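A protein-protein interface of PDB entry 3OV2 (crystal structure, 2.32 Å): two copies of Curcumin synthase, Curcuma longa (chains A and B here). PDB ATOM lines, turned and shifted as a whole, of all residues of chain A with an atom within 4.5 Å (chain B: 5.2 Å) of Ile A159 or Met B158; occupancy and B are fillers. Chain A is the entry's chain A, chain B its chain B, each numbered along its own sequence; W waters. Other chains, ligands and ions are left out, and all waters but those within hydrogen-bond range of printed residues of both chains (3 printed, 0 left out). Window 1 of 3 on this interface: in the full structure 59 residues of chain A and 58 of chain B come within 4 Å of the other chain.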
ATOM      1  N   PHE A 129     -27.111   1.206 -30.878  1.00  0.00           N
ATOM      2  CA  PHE A 129     -28.512   1.414 -30.503  1.00  0.00           C
ATOM      3  C   PHE A 129     -28.698   2.887 -30.188  1.00  0.00           C
ATOM      4  O   PHE A 129     -27.965   3.425 -29.365  1.00  0.00           O
ATOM      5  CB  PHE A 129     -28.847   0.526 -29.283  1.00  0.00           C
ATOM      6  CG  PHE A 129     -30.298   0.610 -28.779  1.00  0.00           C
ATOM      7  CD1 PHE A 129     -31.345   0.999 -29.608  1.00  0.00           C
ATOM      8  CD2 PHE A 129     -30.600   0.235 -27.460  1.00  0.00           C
ATOM      9  CE1 PHE A 129     -32.661   1.051 -29.129  1.00  0.00           C
ATOM     10  CE2 PHE A 129     -31.914   0.285 -26.980  1.00  0.00           C
ATOM     11  CZ  PHE A 129     -32.944   0.712 -27.815  1.00  0.00           C
ATOM     12  N   CYS A 130     -29.647   3.542 -30.877  1.00  0.00           N
ATOM     13  CA  CYS A 130     -29.992   4.922 -30.557  1.00  0.00           C
ATOM     14  C   CYS A 130     -31.442   5.147 -30.138  1.00  0.00           C
ATOM     15  O   CYS A 130     -32.371   4.488 -30.628  1.00  0.00           O
ATOM     16  CB  CYS A 130     -29.613   5.856 -31.710  1.00  0.00           C
ATOM     17  SG  CYS A 130     -30.718   5.799 -33.113  1.00  0.00           S
ATOM     18  N   SER A 131     -31.629   6.074 -29.204  1.00  0.00           N
ATOM     19  CA  SER A 131     -32.947   6.617 -28.894  1.00  0.00           C
ATOM     20  C   SER A 131     -32.795   8.000 -28.264  1.00  0.00           C
ATOM     21  O   SER A 131     -31.772   8.322 -27.669  1.00  0.00           O
ATOM     22  CB  SER A 131     -33.737   5.710 -27.933  1.00  0.00           C
ATOM     23  OG  SER A 131     -35.046   6.246 -27.669  1.00  0.00           O
ATOM     24  N   LEU A 157     -22.849  -0.182 -27.952  1.00  0.00           N
ATOM     25  CA  LEU A 157     -22.767   1.283 -27.998  1.00  0.00           C
ATOM     26  C   LEU A 157     -24.174   1.863 -27.934  1.00  0.00           C
ATOM     27  O   LEU A 157     -25.046   1.458 -28.705  1.00  0.00           O
ATOM     28  CB  LEU A 157     -22.040   1.763 -29.249  1.00  0.00           C
ATOM     29  CG  LEU A 157     -21.905   3.290 -29.375  1.00  0.00           C
ATOM     30  CD1 LEU A 157     -21.106   3.926 -28.208  1.00  0.00           C
ATOM     31  CD2 LEU A 157     -21.308   3.657 -30.706  1.00  0.00           C
ATOM     32  N   MET A 158     -24.412   2.766 -26.975  1.00  0.00           N
ATOM     33  CA  MET A 158     -25.717   3.423 -26.831  1.00  0.00           C
ATOM     34  C   MET A 158     -25.584   4.896 -27.173  1.00  0.00           C
ATOM     35  O   MET A 158     -24.732   5.617 -26.600  1.00  0.00           O
ATOM     36  CB  MET A 158     -26.268   3.272 -25.413  1.00  0.00           C
ATOM     37  CG  MET A 158     -27.658   3.876 -25.216  1.00  0.00           C
ATOM     38  SD  MET A 158     -28.912   2.809 -25.949  1.00  0.00           S
ATOM     39  CE  MET A 158     -29.922   4.005 -26.853  1.00  0.00           C
ATOM     40  N   ILE A 159     -26.424   5.345 -28.096  1.00  0.00           N
ATOM     41  CA  ILE A 159     -26.436   6.744 -28.495  1.00  0.00           C
ATOM     42  C   ILE A 159     -27.745   7.378 -28.008  1.00  0.00           C
ATOM     43  O   ILE A 159     -28.794   7.167 -28.608  1.00  0.00           O
ATOM     44  CB  ILE A 159     -26.324   6.912 -30.052  1.00  0.00           C
ATOM     45  CG1 ILE A 159     -25.300   5.931 -30.681  1.00  0.00           C
ATOM     46  CG2 ILE A 159     -26.032   8.379 -30.424  1.00  0.00           C
ATOM     47  CD1 ILE A 159     -23.895   6.107 -30.168  1.00  0.00           C
ATOM     48  N   TYR A 160     -27.677   8.168 -26.938  1.00  0.00           N
ATOM     49  CA  TYR A 160     -28.879   8.742 -26.343  1.00  0.00           C
ATOM     50  C   TYR A 160     -29.121  10.178 -26.805  1.00  0.00           C
ATOM     51  O   TYR A 160     -28.179  10.987 -26.905  1.00  0.00           O
ATOM     52  CB  TYR A 160     -28.772   8.778 -24.811  1.00  0.00           C
ATOM     53  CG  TYR A 160     -29.169   7.542 -24.023  1.00  0.00           C
ATOM     54  CD1 TYR A 160     -30.444   6.986 -24.131  1.00  0.00           C
ATOM     55  CD2 TYR A 160     -28.285   6.986 -23.096  1.00  0.00           C
ATOM     56  CE1 TYR A 160     -30.798   5.851 -23.374  1.00  0.00           C
ATOM     57  CE2 TYR A 160     -28.627   5.891 -22.330  1.00  0.00           C
ATOM     58  CZ  TYR A 160     -29.890   5.323 -22.471  1.00  0.00           C
ATOM     59  OH  TYR A 160     -30.234   4.227 -21.701  1.00  0.00           O
ATOM     60  N   SER A 161     -30.386  10.504 -27.046  1.00  0.00           N
ATOM     61  CA  SER A 161     -30.824  11.908 -27.065  1.00  0.00           C
ATOM     62  C   SER A 161     -30.268  12.733 -28.232  1.00  0.00           C
ATOM     63  O   SER A 161     -30.141  13.960 -28.149  1.00  0.00           O
ATOM     64  CB  SER A 161     -30.513  12.590 -25.711  1.00  0.00           C
ATOM     65  OG  SER A 161     -31.290  12.026 -24.672  1.00  0.00           O
ATOM     66  N   GLN A 162     -29.951  12.050 -29.321  1.00  0.00           N
ATOM     67  CA  GLN A 162     -29.635  12.728 -30.559  1.00  0.00           C
ATOM     68  C   GLN A 162     -30.933  12.798 -31.338  1.00  0.00           C
ATOM     69  O   GLN A 162     -31.807  11.950 -31.167  1.00  0.00           O
ATOM     70  CB  GLN A 162     -28.541  11.966 -31.331  1.00  0.00           C
ATOM     71  CG  GLN A 162     -27.224  11.840 -30.553  1.00  0.00           C
ATOM     72  CD  GLN A 162     -26.705  13.180 -30.026  1.00  0.00           C
ATOM     73  OE1 GLN A 162     -26.589  13.384 -28.814  1.00  0.00           O
ATOM     74  NE2 GLN A 162     -26.404  14.099 -30.928  1.00  0.00           N
ATOM     75  N   MET A 166     -30.258  10.911 -36.390  1.00  0.00           N
ATOM     76  CA  MET A 166     -29.436   9.865 -35.784  1.00  0.00           C
ATOM     77  C   MET A 166     -29.598   8.490 -36.428  1.00  0.00           C
ATOM     78  O   MET A 166     -28.672   7.674 -36.385  1.00  0.00           O
ATOM     79  CB  MET A 166     -29.650   9.775 -34.268  1.00  0.00           C
ATOM     80  CG  MET A 166     -28.558   8.967 -33.537  1.00  0.00           C
ATOM     81  SD  MET A 166     -26.869   9.669 -33.712  1.00  0.00           S
ATOM     82  CE  MET A 166     -26.005   8.164 -34.165  1.00  0.00           C
ATOM     83  N   ILE A 173     -21.768   5.151 -38.538  1.00  0.00           N
ATOM     84  CA  ILE A 173     -21.023   4.415 -37.533  1.00  0.00           C
ATOM     85  C   ILE A 173     -20.809   2.972 -37.990  1.00  0.00           C
ATOM     86  O   ILE A 173     -19.676   2.521 -38.099  1.00  0.00           O
ATOM     87  CB  ILE A 173     -21.743   4.438 -36.169  1.00  0.00           C
ATOM     88  CG1 ILE A 173     -21.841   5.863 -35.635  1.00  0.00           C
ATOM     89  CG2 ILE A 173     -21.015   3.556 -35.144  1.00  0.00           C
ATOM     90  CD1 ILE A 173     -22.855   5.972 -34.472  1.00  0.00           C
ATOM     91  N   PHE B 129     -17.259  12.688 -28.718  1.00  0.00           N
ATOM     92  CA  PHE B 129     -17.381  13.419 -27.444  1.00  0.00           C
ATOM     93  C   PHE B 129     -18.337  12.699 -26.457  1.00  0.00           C
ATOM     94  O   PHE B 129     -19.474  12.384 -26.791  1.00  0.00           O
ATOM     95  CB  PHE B 129     -17.817  14.854 -27.783  1.00  0.00           C
ATOM     96  CG  PHE B 129     -17.973  15.781 -26.601  1.00  0.00           C
ATOM     97  CD1 PHE B 129     -17.256  15.607 -25.428  1.00  0.00           C
ATOM     98  CD2 PHE B 129     -18.812  16.890 -26.711  1.00  0.00           C
ATOM     99  CE1 PHE B 129     -17.430  16.491 -24.365  1.00  0.00           C
ATOM    100  CE2 PHE B 129     -18.970  17.763 -25.666  1.00  0.00           C
ATOM    101  CZ  PHE B 129     -18.287  17.556 -24.492  1.00  0.00           C
ATOM    102  N   CYS B 130     -17.851  12.378 -25.256  1.00  0.00           N
ATOM    103  CA  CYS B 130     -18.718  11.743 -24.266  1.00  0.00           C
ATOM    104  C   CYS B 130     -18.850  12.557 -22.993  1.00  0.00           C
ATOM    105  O   CYS B 130     -17.902  13.224 -22.571  1.00  0.00           O
ATOM    106  CB  CYS B 130     -18.274  10.315 -23.961  1.00  0.00           C
ATOM    107  SG  CYS B 130     -16.814  10.150 -22.900  1.00  0.00           S
ATOM    108  N   SER B 131     -20.042  12.512 -22.402  1.00  0.00           N
ATOM    109  CA  SER B 131     -20.291  13.062 -21.066  1.00  0.00           C
ATOM    110  C   SER B 131     -21.542  12.467 -20.471  1.00  0.00           C
ATOM    111  O   SER B 131     -22.451  12.132 -21.176  1.00  0.00           O
ATOM    112  CB  SER B 131     -20.440  14.591 -21.078  1.00  0.00           C
ATOM    113  OG  SER B 131     -20.746  15.071 -19.761  1.00  0.00           O
ATOM    114  N   SER B 133     -23.427  14.325 -18.794  1.00  0.00           N
ATOM    115  CA  SER B 133     -24.297  15.484 -18.639  1.00  0.00           C
ATOM    116  C   SER B 133     -24.355  16.373 -19.878  1.00  0.00           C
ATOM    117  O   SER B 133     -23.590  16.182 -20.840  1.00  0.00           O
ATOM    118  CB  SER B 133     -23.798  16.310 -17.466  1.00  0.00           C
ATOM    119  OG  SER B 133     -23.439  15.457 -16.385  1.00  0.00           O
ATOM    120  N   ALA B 140     -24.165  18.785 -26.967  1.00  0.00           N
ATOM    121  CA  ALA B 140     -22.879  19.243 -26.453  1.00  0.00           C
ATOM    122  C   ALA B 140     -21.785  19.176 -27.524  1.00  0.00           C
ATOM    123  O   ALA B 140     -20.871  19.988 -27.507  1.00  0.00           O
ATOM    124  CB  ALA B 140     -22.484  18.407 -25.218  1.00  0.00           C
ATOM    125  N   ASP B 141     -21.893  18.223 -28.456  1.00  0.00           N
ATOM    126  CA  ASP B 141     -20.878  18.053 -29.507  1.00  0.00           C
ATOM    127  C   ASP B 141     -20.910  19.239 -30.463  1.00  0.00           C
ATOM    128  O   ASP B 141     -19.855  19.751 -30.871  1.00  0.00           O
ATOM    129  CB  ASP B 141     -21.061  16.729 -30.288  1.00  0.00           C
ATOM    130  CG  ASP B 141     -22.441  16.605 -30.900  1.00  0.00           C
ATOM    131  OD1 ASP B 141     -23.422  16.755 -30.158  1.00  0.00           O
ATOM    132  OD2 ASP B 141     -22.568  16.379 -32.118  1.00  0.00           O
ATOM    133  N   ARG B 156     -19.489  14.393 -36.370  1.00  0.00           N
ATOM    134  CA  ARG B 156     -19.613  14.452 -34.909  1.00  0.00           C
ATOM    135  C   ARG B 156     -20.378  13.266 -34.399  1.00  0.00           C
ATOM    136  O   ARG B 156     -21.333  12.831 -35.040  1.00  0.00           O
ATOM    137  CB  ARG B 156     -20.357  15.689 -34.438  1.00  0.00           C
ATOM    138  CG  ARG B 156     -19.777  16.990 -34.861  1.00  0.00           C
ATOM    139  CD  ARG B 156     -20.639  18.111 -34.332  1.00  0.00           C
ATOM    140  NE  ARG B 156     -21.681  18.525 -35.277  1.00  0.00           N
ATOM    141  CZ  ARG B 156     -22.984  18.239 -35.180  1.00  0.00           C
ATOM    142  NH1 ARG B 156     -23.446  17.508 -34.167  1.00  0.00           N
ATOM    143  NH2 ARG B 156     -23.828  18.695 -36.116  1.00  0.00           N
ATOM    144  N   LEU B 157     -19.959  12.762 -33.245  1.00  0.00           N
ATOM    145  CA  LEU B 157     -20.746  11.814 -32.498  1.00  0.00           C
ATOM    146  C   LEU B 157     -20.735  12.149 -31.017  1.00  0.00           C
ATOM    147  O   LEU B 157     -19.690  12.131 -30.386  1.00  0.00           O
ATOM    148  CB  LEU B 157     -20.230  10.389 -32.708  1.00  0.00           C
ATOM    149  CG  LEU B 157     -20.988   9.366 -31.861  1.00  0.00           C
ATOM    150  CD1 LEU B 157     -22.346   9.074 -32.500  1.00  0.00           C
ATOM    151  CD2 LEU B 157     -20.167   8.102 -31.648  1.00  0.00           C
ATOM    152  N   MET B 158     -21.909  12.446 -30.467  1.00  0.00           N
ATOM    153  CA  MET B 158     -22.070  12.657 -29.033  1.00  0.00           C
ATOM    154  C   MET B 158     -22.547  11.375 -28.382  1.00  0.00           C
ATOM    155  O   MET B 158     -23.507  10.748 -28.863  1.00  0.00           O
ATOM    156  CB  MET B 158     -23.084  13.762 -28.759  1.00  0.00           C
ATOM    157  CG  MET B 158     -23.207  14.134 -27.285  1.00  0.00           C
ATOM    158  SD  MET B 158     -21.809  15.130 -26.754  1.00  0.00           S
ATOM    159  CE  MET B 158     -21.497  14.414 -25.114  1.00  0.00           C
ATOM    160  N   ILE B 159     -21.875  10.996 -27.286  1.00  0.00           N
ATOM    161  CA  ILE B 159     -22.292   9.876 -26.446  1.00  0.00           C
ATOM    162  C   ILE B 159     -22.615  10.357 -25.022  1.00  0.00           C
ATOM    163  O   ILE B 159     -21.712  10.537 -24.186  1.00  0.00           O
ATOM    164  CB  ILE B 159     -21.226   8.759 -26.371  1.00  0.00           C
ATOM    165  CG1 ILE B 159     -20.853   8.259 -27.766  1.00  0.00           C
ATOM    166  CG2 ILE B 159     -21.739   7.603 -25.568  1.00  0.00           C
ATOM    167  CD1 ILE B 159     -19.462   8.557 -28.129  1.00  0.00           C
ATOM    168  N   TYR B 160     -23.913  10.500 -24.749  1.00  0.00           N
ATOM    169  CA  TYR B 160     -24.402  10.978 -23.481  1.00  0.00           C
ATOM    170  C   TYR B 160     -24.623   9.859 -22.474  1.00  0.00           C
ATOM    171  O   TYR B 160     -25.048   8.737 -22.830  1.00  0.00           O
ATOM    172  CB  TYR B 160     -25.738  11.702 -23.673  1.00  0.00           C
ATOM    173  CG  TYR B 160     -25.702  13.159 -24.149  1.00  0.00           C
ATOM    174  CD1 TYR B 160     -25.026  14.148 -23.434  1.00  0.00           C
ATOM    175  CD2 TYR B 160     -26.405  13.544 -25.272  1.00  0.00           C
ATOM    176  CE1 TYR B 160     -25.036  15.476 -23.864  1.00  0.00           C
ATOM    177  CE2 TYR B 160     -26.427  14.866 -25.706  1.00  0.00           C
ATOM    178  CZ  TYR B 160     -25.742  15.824 -24.994  1.00  0.00           C
ATOM    179  OH  TYR B 160     -25.773  17.130 -25.431  1.00  0.00           O
HETATM  180  O   HOH W   1     -25.395  10.541 -27.040  1.00  0.00           O
HETATM  181  O   HOH W   2     -25.259   7.680 -25.238  1.00  0.00           O
HETATM  182  O   HOH W   3     -26.024  17.414 -31.521  1.00  0.00           O
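The backbone NH of Ile A159 sits at hydrogen-bond distance from the backbone carbonyl oxygen of Phe A129.
The backbone NH (N) of Ser A131 is in hydrogen-bond range of the backbone carbonyl oxygen (O) of Ile A159 (3.1 Å).
OE1 of Gln A162 sits close to O of Tyr A160.
The backbone carbonyl oxygen of Phe B129 sits at hydrogen-bond distance from the backbone NH of Ile B159.
O of Ile B159 sits at hydrogen-bond distance from N of Ser B131 (3.1 Å).
SD of Met B158 sits at hydrogen-bond distance from N of Asp B141, at 3.5 Å.
Among the printed residues, pairs that only touch across the chains: Gln A162 with Tyr B160 (3.4 Å), Tyr A160 with Tyr B160 (3.5 Å), Gln A162 with Met B158 (3.5 Å), Ile A173 with Leu B157 (3.7 Å), Met A158 with Ile B159 (3.7 Å) and Ile A159 with Met B158 (3.8 Å).
Of chain B, only Met B158 comes within 4 Å of Ile A159.
Of chain A, only Ile A159 (3.8 Å) and Gln A162 (3.5 Å) come within 4 Å of Met B158.
Printed residues of chain A within 4 Å of Leu B157: Ile A173 (3.7 Å).
Of the printed residues of chain A, Tyr B160 touches Tyr A160 (3.5 Å) and Gln A162 (3.4 Å).
Of the printed residues of chain B, Tyr A160 touches Tyr B160 (3.5 Å).
Of the printed residues of chain B, Gln A162 touches Met B158 (3.5 Å) and Tyr B160 (3.4 Å).
Phe A129 touches none of the printed residues of chain B.
The nearest residue of chain B that does not touch Ile A159 is Leu B157 (4.1 Å).
Printed residues of chain A that touch a printed residue of chain B: Met A158, Ile A159, Tyr A160, Gln A162 and Ile A173.
Hydrophobic or aromatic side chains of chain B within 4 Å of the printed part of chain A: Leu B157, Met B158, Ile B159 and Tyr B160.
Among the printed residues, 6 pairs touch across the chains.
Among the printed residues, no Asp or Glu carboxylate lies within 4 Å of a Lys or Arg side-chain nitrogen of the other chain.
Met A158 touches Ile B159, and with the chains exchanged Ile A159 touches Met B158.
Tyr B160 touches its own counterpart, Tyr A160.
Positions printed for both chains: 129, 130, 131, 157, 158, 159 and 160.
Water W2 lies within hydrogen-bond range of O of Met A158 (2.5 Å), O of Tyr B160 (2.6 Å) and N of Tyr A160 (3.0 Å).
Water W1 lies within hydrogen-bond range of O of Met B158 (2.6 Å), N of Tyr B160 (2.7 Å) and O of Tyr A160 (2.8 Å).
Water W3 lies within hydrogen-bond range of the side-chain carboxylate (OD1) of Asp B141 (3.0 Å) and the side-chain amide nitrogen (NE2) of Gln A162 (3.4 Å).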
